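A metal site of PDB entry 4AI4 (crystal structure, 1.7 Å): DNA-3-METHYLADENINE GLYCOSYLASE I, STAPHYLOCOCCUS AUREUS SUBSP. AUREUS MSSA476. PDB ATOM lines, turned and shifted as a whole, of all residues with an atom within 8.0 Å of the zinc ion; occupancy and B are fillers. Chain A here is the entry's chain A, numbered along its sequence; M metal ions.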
ATOM      1  N   MET A   3      -1.035 -21.959 -17.783  1.00  0.00           N
ATOM      2  CA  MET A   3      -2.333 -21.205 -17.702  1.00  0.00           C
ATOM      3  C   MET A   3      -2.075 -19.773 -17.285  1.00  0.00           C
ATOM      4  O   MET A   3      -2.610 -18.857 -17.902  1.00  0.00           O
ATOM      5  CB  MET A   3      -3.307 -21.850 -16.698  1.00  0.00           C
ATOM      6  CG  MET A   3      -4.684 -21.196 -16.612  1.00  0.00           C
ATOM      7  SD  MET A   3      -4.926 -19.855 -15.407  1.00  0.00           S
ATOM      8  CE  MET A   3      -4.609 -20.662 -13.828  1.00  0.00           C
ATOM      9  N   ASN A   4      -1.285 -19.577 -16.220  1.00  0.00           N
ATOM     10  CA  ASN A   4      -1.045 -18.217 -15.680  1.00  0.00           C
ATOM     11  C   ASN A   4      -0.418 -17.298 -16.715  1.00  0.00           C
ATOM     12  O   ASN A   4      -0.839 -16.143 -16.872  1.00  0.00           O
ATOM     13  CB  ASN A   4      -0.133 -18.226 -14.453  1.00  0.00           C
ATOM     14  CG  ASN A   4       0.322 -16.809 -14.071  1.00  0.00           C
ATOM     15  OD1 ASN A   4      -0.485 -15.964 -13.628  1.00  0.00           O
ATOM     16  ND2 ASN A   4       1.615 -16.526 -14.257  1.00  0.00           N
ATOM     17  N   GLU A   5       0.577 -17.794 -17.434  1.00  0.00           N
ATOM     18  CA  GLU A   5       1.206 -16.977 -18.468  1.00  0.00           C
ATOM     19  C   GLU A   5       0.219 -16.613 -19.557  1.00  0.00           C
ATOM     20  O   GLU A   5       0.212 -15.478 -20.031  1.00  0.00           O
ATOM     21  CB  GLU A   5       2.422 -17.678 -19.097  1.00  0.00           C
ATOM     22  CG  GLU A   5       3.109 -16.778 -20.111  1.00  0.00           C
ATOM     23  CD  GLU A   5       4.270 -17.425 -20.804  1.00  0.00           C
ATOM     24  OE1 GLU A   5       4.537 -18.610 -20.515  1.00  0.00           O
ATOM     25  OE2 GLU A   5       4.912 -16.741 -21.634  1.00  0.00           O
ATOM     26  N   CYS A   6      -0.589 -17.595 -19.975  1.00  0.00           N
ATOM     27  CA  CYS A   6      -1.575 -17.382 -21.014  1.00  0.00           C
ATOM     28  C   CYS A   6      -2.591 -16.316 -20.601  1.00  0.00           C
ATOM     29  O   CYS A   6      -2.974 -15.460 -21.408  1.00  0.00           O
ATOM     30  CB  CYS A   6      -2.310 -18.675 -21.368  1.00  0.00           C
ATOM     31  SG  CYS A   6      -3.320 -18.521 -22.889  1.00  0.00           S
ATOM     32  N   ALA A   7      -3.041 -16.400 -19.344  1.00  0.00           N
ATOM     33  CA  ALA A   7      -4.037 -15.470 -18.801  1.00  0.00           C
ATOM     34  C   ALA A   7      -3.448 -14.096 -18.376  1.00  0.00           C
ATOM     35  O   ALA A   7      -4.050 -13.409 -17.548  1.00  0.00           O
ATOM     36  CB  ALA A   7      -4.772 -16.133 -17.629  1.00  0.00           C
ATOM     37  N   PHE A   8      -2.295 -13.706 -18.934  1.00  0.00           N
ATOM     38  CA  PHE A   8      -1.713 -12.359 -18.706  1.00  0.00           C
ATOM     39  C   PHE A   8      -1.325 -12.061 -17.256  1.00  0.00           C
ATOM     40  O   PHE A   8      -1.361 -10.901 -16.825  1.00  0.00           O
ATOM     41  CB  PHE A   8      -2.691 -11.271 -19.183  1.00  0.00           C
ATOM     42  CG  PHE A   8      -2.991 -11.289 -20.646  1.00  0.00           C
ATOM     43  CD1 PHE A   8      -3.943 -12.149 -21.169  1.00  0.00           C
ATOM     44  CD2 PHE A   8      -2.359 -10.393 -21.520  1.00  0.00           C
ATOM     45  CE1 PHE A   8      -4.227 -12.161 -22.524  1.00  0.00           C
ATOM     46  CE2 PHE A   8      -2.633 -10.398 -22.882  1.00  0.00           C
ATOM     47  CZ  PHE A   8      -3.579 -11.284 -23.380  1.00  0.00           C
ATOM     48  N   HIS A  19     -11.045 -16.171 -19.125  1.00  0.00           N
ATOM     49  CA  HIS A  19      -9.979 -16.791 -19.894  1.00  0.00           C
ATOM     50  C   HIS A  19     -10.230 -18.262 -20.133  1.00  0.00           C
ATOM     51  O   HIS A  19      -9.931 -18.793 -21.220  1.00  0.00           O
ATOM     52  CB  HIS A  19      -8.624 -16.631 -19.229  1.00  0.00           C
ATOM     53  CG  HIS A  19      -7.609 -17.615 -19.744  1.00  0.00           C
ATOM     54  ND1 HIS A  19      -7.467 -18.833 -19.206  1.00  0.00           N
ATOM     55  CD2 HIS A  19      -6.785 -17.589 -20.852  1.00  0.00           C
ATOM     56  CE1 HIS A  19      -6.572 -19.535 -19.912  1.00  0.00           C
ATOM     57  NE2 HIS A  19      -6.140 -18.772 -20.909  1.00  0.00           N
ATOM     58  N   ASP A  20     -10.756 -18.928 -19.117  1.00  0.00           N
ATOM     59  CA  ASP A  20     -10.853 -20.381 -19.093  1.00  0.00           C
ATOM     60  C   ASP A  20     -12.063 -20.885 -19.885  1.00  0.00           C
ATOM     61  O   ASP A  20     -12.024 -22.016 -20.381  1.00  0.00           O
ATOM     62  CB  ASP A  20     -11.004 -20.923 -17.676  1.00  0.00           C
ATOM     63  CG  ASP A  20      -9.715 -20.887 -16.824  1.00  0.00           C
ATOM     64  OD1 ASP A  20      -8.603 -20.481 -17.245  1.00  0.00           O
ATOM     65  OD2 ASP A  20      -9.856 -21.273 -15.653  1.00  0.00           O
ATOM     66  N   TRP A  23     -12.861 -16.836 -23.550  1.00  0.00           N
ATOM     67  CA  TRP A  23     -11.848 -16.248 -24.421  1.00  0.00           C
ATOM     68  C   TRP A  23     -11.233 -17.275 -25.348  1.00  0.00           C
ATOM     69  O   TRP A  23     -10.692 -18.311 -24.891  1.00  0.00           O
ATOM     70  CB  TRP A  23     -10.762 -15.580 -23.573  1.00  0.00           C
ATOM     71  CG  TRP A  23      -9.798 -14.716 -24.357  1.00  0.00           C
ATOM     72  CD1 TRP A  23     -10.021 -13.452 -24.880  1.00  0.00           C
ATOM     73  CD2 TRP A  23      -8.404 -15.018 -24.673  1.00  0.00           C
ATOM     74  NE1 TRP A  23      -8.884 -12.974 -25.497  1.00  0.00           N
ATOM     75  CE2 TRP A  23      -7.889 -13.869 -25.411  1.00  0.00           C
ATOM     76  CE3 TRP A  23      -7.552 -16.087 -24.412  1.00  0.00           C
ATOM     77  CZ2 TRP A  23      -6.559 -13.814 -25.870  1.00  0.00           C
ATOM     78  CZ3 TRP A  23      -6.242 -16.025 -24.892  1.00  0.00           C
ATOM     79  CH2 TRP A  23      -5.758 -14.924 -25.596  1.00  0.00           C
ATOM     80  N   GLY A  24     -11.324 -17.048 -26.653  1.00  0.00           N
ATOM     81  CA  GLY A  24     -10.684 -17.916 -27.614  1.00  0.00           C
ATOM     82  C   GLY A  24     -11.411 -19.208 -27.956  1.00  0.00           C
ATOM     83  O   GLY A  24     -10.912 -20.003 -28.754  1.00  0.00           O
ATOM     84  N   GLN A  25     -12.580 -19.449 -27.336  1.00  0.00           N
ATOM     85  CA  GLN A  25     -13.387 -20.626 -27.706  1.00  0.00           C
ATOM     86  C   GLN A  25     -14.244 -20.230 -28.887  1.00  0.00           C
ATOM     87  O   GLN A  25     -15.008 -19.266 -28.802  1.00  0.00           O
ATOM     88  CB  GLN A  25     -14.287 -21.115 -26.564  1.00  0.00           C
ATOM     89  CG  GLN A  25     -13.539 -21.343 -25.261  1.00  0.00           C
ATOM     90  CD  GLN A  25     -12.444 -22.389 -25.387  1.00  0.00           C
ATOM     91  OE1 GLN A  25     -12.550 -23.314 -26.194  1.00  0.00           O
ATOM     92  NE2 GLN A  25     -11.391 -22.238 -24.621  1.00  0.00           N
ATOM     93  N   ARG A 137       2.527 -12.298 -28.477  1.00  0.00           N
ATOM     94  CA  ARG A 137       1.216 -11.747 -28.834  1.00  0.00           C
ATOM     95  C   ARG A 137       1.219 -10.321 -29.390  1.00  0.00           C
ATOM     96  O   ARG A 137       1.714  -9.398 -28.782  1.00  0.00           O
ATOM     97  CB  ARG A 137       0.296 -11.810 -27.632  1.00  0.00           C
ATOM     98  CG  ARG A 137       0.014 -13.225 -27.155  1.00  0.00           C
ATOM     99  CD  ARG A 137      -1.122 -13.136 -26.194  1.00  0.00           C
ATOM    100  NE  ARG A 137      -1.635 -14.418 -25.766  1.00  0.00           N
ATOM    101  CZ  ARG A 137      -1.784 -14.783 -24.507  1.00  0.00           C
ATOM    102  NH1 ARG A 137      -1.428 -13.970 -23.496  1.00  0.00           N
ATOM    103  NH2 ARG A 137      -2.282 -15.957 -24.256  1.00  0.00           N
ATOM    104  N   ASP A 175      -7.199 -17.862 -32.303  1.00  0.00           N
ATOM    105  CA  ASP A 175      -6.860 -18.571 -31.092  1.00  0.00           C
ATOM    106  C   ASP A 175      -5.485 -18.075 -30.682  1.00  0.00           C
ATOM    107  O   ASP A 175      -4.481 -18.434 -31.329  1.00  0.00           O
ATOM    108  CB  ASP A 175      -6.852 -20.074 -31.354  1.00  0.00           C
ATOM    109  CG  ASP A 175      -6.259 -20.894 -30.231  1.00  0.00           C
ATOM    110  OD1 ASP A 175      -5.884 -20.315 -29.172  1.00  0.00           O
ATOM    111  OD2 ASP A 175      -6.160 -22.126 -30.414  1.00  0.00           O
ATOM    112  N   ALA A 176      -5.492 -17.212 -29.665  1.00  0.00           N
ATOM    113  CA  ALA A 176      -4.305 -16.602 -29.075  1.00  0.00           C
ATOM    114  C   ALA A 176      -3.871 -17.316 -27.781  1.00  0.00           C
ATOM    115  O   ALA A 176      -2.990 -16.816 -27.067  1.00  0.00           O
ATOM    116  CB  ALA A 176      -4.547 -15.109 -28.851  1.00  0.00           C
ATOM    117  N   HIS A 177      -4.446 -18.475 -27.471  1.00  0.00           N
ATOM    118  CA  HIS A 177      -3.980 -19.252 -26.328  1.00  0.00           C
ATOM    119  C   HIS A 177      -2.595 -19.819 -26.565  1.00  0.00           C
ATOM    120  O   HIS A 177      -2.240 -20.233 -27.686  1.00  0.00           O
ATOM    121  CB  HIS A 177      -4.900 -20.437 -25.990  1.00  0.00           C
ATOM    122  CG  HIS A 177      -6.197 -20.064 -25.371  1.00  0.00           C
ATOM    123  ND1 HIS A 177      -6.342 -19.819 -24.047  1.00  0.00           N
ATOM    124  CD2 HIS A 177      -7.444 -19.878 -25.943  1.00  0.00           C
ATOM    125  CE1 HIS A 177      -7.631 -19.540 -23.790  1.00  0.00           C
ATOM    126  NE2 HIS A 177      -8.305 -19.575 -24.941  1.00  0.00           N
ATOM    127  N   LEU A 178      -1.812 -19.906 -25.490  1.00  0.00           N
ATOM    128  CA  LEU A 178      -0.481 -20.499 -25.593  1.00  0.00           C
ATOM    129  C   LEU A 178      -0.592 -22.018 -25.758  1.00  0.00           C
ATOM    130  O   LEU A 178      -1.548 -22.644 -25.280  1.00  0.00           O
ATOM    131  CB  LEU A 178       0.367 -20.148 -24.372  1.00  0.00           C
ATOM    132  CG  LEU A 178       0.521 -18.652 -24.063  1.00  0.00           C
ATOM    133  CD1 LEU A 178       1.548 -18.458 -22.952  1.00  0.00           C
ATOM    134  CD2 LEU A 178       0.874 -17.841 -25.295  1.00  0.00           C
ATOM    135  N   LYS A 179       0.425 -22.579 -26.399  1.00  0.00           N
ATOM    136  CA  LYS A 179       0.464 -23.994 -26.769  1.00  0.00           C
ATOM    137  C   LYS A 179       0.121 -24.932 -25.614  1.00  0.00           C
ATOM    138  O   LYS A 179      -0.661 -25.875 -25.797  1.00  0.00           O
ATOM    139  CB  LYS A 179       1.849 -24.328 -27.356  1.00  0.00           C
ATOM    140  CG  LYS A 179       2.081 -25.787 -27.697  1.00  0.00           C
ATOM    141  CD  LYS A 179       3.324 -25.930 -28.579  1.00  0.00           C
ATOM    142  CE  LYS A 179       3.687 -27.376 -28.880  1.00  0.00           C
ATOM    143  NZ  LYS A 179       4.955 -27.489 -29.688  1.00  0.00           N
ATOM    144  N   ASP A 180       0.674 -24.679 -24.432  1.00  0.00           N
ATOM    145  CA  ASP A 180       0.423 -25.524 -23.272  1.00  0.00           C
ATOM    146  C   ASP A 180      -0.682 -25.038 -22.316  1.00  0.00           C
ATOM    147  O   ASP A 180      -0.879 -25.613 -21.249  1.00  0.00           O
ATOM    148  CB  ASP A 180       1.738 -25.722 -22.497  1.00  0.00           C
ATOM    149  CG  ASP A 180       2.812 -26.405 -23.325  1.00  0.00           C
ATOM    150  OD1 ASP A 180       2.487 -27.275 -24.171  1.00  0.00           O
ATOM    151  OD2 ASP A 180       3.999 -26.050 -23.124  1.00  0.00           O
ATOM    152  N   CYS A 181      -1.421 -23.988 -22.685  1.00  0.00           N
ATOM    153  CA  CYS A 181      -2.565 -23.578 -21.882  1.00  0.00           C
ATOM    154  C   CYS A 181      -3.616 -24.694 -21.883  1.00  0.00           C
ATOM    155  O   CYS A 181      -3.975 -25.206 -22.952  1.00  0.00           O
ATOM    156  CB  CYS A 181      -3.212 -22.307 -22.448  1.00  0.00           C
ATOM    157  SG  CYS A 181      -4.560 -21.787 -21.393  1.00  0.00           S
ATOM    158  N   PRO A 182      -4.145 -25.057 -20.695  1.00  0.00           N
ATOM    159  CA  PRO A 182      -5.221 -26.069 -20.605  1.00  0.00           C
ATOM    160  C   PRO A 182      -6.529 -25.672 -21.279  1.00  0.00           C
ATOM    161  O   PRO A 182      -7.420 -26.518 -21.383  1.00  0.00           O
ATOM    162  CB  PRO A 182      -5.477 -26.215 -19.094  1.00  0.00           C
ATOM    163  CG  PRO A 182      -4.397 -25.478 -18.404  1.00  0.00           C
ATOM    164  CD  PRO A 182      -3.767 -24.527 -19.367  1.00  0.00           C
ATOM    165  N   SER A 183      -6.669 -24.399 -21.654  1.00  0.00           N
ATOM    166  CA  SER A 183      -7.869 -23.904 -22.309  1.00  0.00           C
ATOM    167  C   SER A 183      -7.651 -23.694 -23.785  1.00  0.00           C
ATOM    168  O   SER A 183      -8.521 -23.149 -24.453  1.00  0.00           O
ATOM    169  CB  SER A 183      -8.335 -22.597 -21.651  1.00  0.00           C
ATOM    170  OG  SER A 183      -8.855 -22.887 -20.357  1.00  0.00           O
ATOM    171  N   LYS A 184      -6.506 -24.096 -24.325  1.00  0.00           N
ATOM    172  CA  LYS A 184      -6.311 -23.976 -25.766  1.00  0.00           C
ATOM    173  C   LYS A 184      -7.257 -24.933 -26.496  1.00  0.00           C
ATOM    174  O   LYS A 184      -7.246 -26.147 -26.264  1.00  0.00           O
ATOM    175  CB  LYS A 184      -4.860 -24.242 -26.201  1.00  0.00           C
ATOM    176  CG  LYS A 184      -4.707 -23.915 -27.681  1.00  0.00           C
ATOM    177  CD  LYS A 184      -3.297 -23.997 -28.161  1.00  0.00           C
ATOM    178  CE  LYS A 184      -3.237 -23.705 -29.651  1.00  0.00           C
ATOM    179  NZ  LYS A 184      -3.237 -22.237 -29.953  1.00  0.00           N
ATOM    180  N   PRO A 185      -8.129 -24.375 -27.369  1.00  0.00           N
ATOM    181  CA  PRO A 185      -9.076 -25.250 -28.063  1.00  0.00           C
ATOM    182  C   PRO A 185      -8.397 -26.178 -29.069  1.00  0.00           C
ATOM    183  O   PRO A 185      -7.322 -25.862 -29.583  1.00  0.00           O
ATOM    184  CB  PRO A 185     -10.021 -24.267 -28.799  1.00  0.00           C
ATOM    185  CG  PRO A 185      -9.373 -22.949 -28.740  1.00  0.00           C
ATOM    186  CD  PRO A 185      -8.307 -22.950 -27.693  1.00  0.00           C
HETATM  187 ZN    ZN M   1      -5.047 -19.768 -22.372  1.00  0.00          ZN
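Four residues have an atom within 4 Å of the zinc ion: Cys 6, His 19, His 177 and Cys 181. The nearest printed residue that does not touch the zinc ion is Ser 183 (4.4 Å).
A ring nitrogen (NE2) of His 19 binds the zinc ion, 2.1 Å away. ND1 of His 177 is bound to the zinc ion, at 2.1 Å. The side-chain sulfur (SG) of Cys 6 is bound to the zinc ion, 2.2 Å away. The zinc ion is bound by the side-chain sulfur (SG) of Cys 181, at 2.3 Å. The zinc ion has four donor atoms within binding distance.
A ring nitrogen (ND1) of His 19 is in hydrogen-bond range of the side-chain carboxylate (OD1) of Asp 20, at 2.8 Å. NE2 of His 177 is in hydrogen-bond range of O of Trp 23 (2.7 Å). O of His 177 sits at hydrogen-bond distance from NZ of Lys 184, 3.2 Å away. The backbone NH (N) of His 177 lies within hydrogen-bond range of the side-chain carboxylate (OD1) of Asp 175. The side-chain sulfur (SG) of Cys 6 sits close to the backbone NH (N) of Leu 178 (3.3 Å). NH2 of Arg 137 lies within hydrogen-bond range of O of Cys 6 (3.0 Å). The backbone NH (N) of Ser 183 lies close to the side-chain sulfur (SG) of Cys 181 (3.4 Å).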
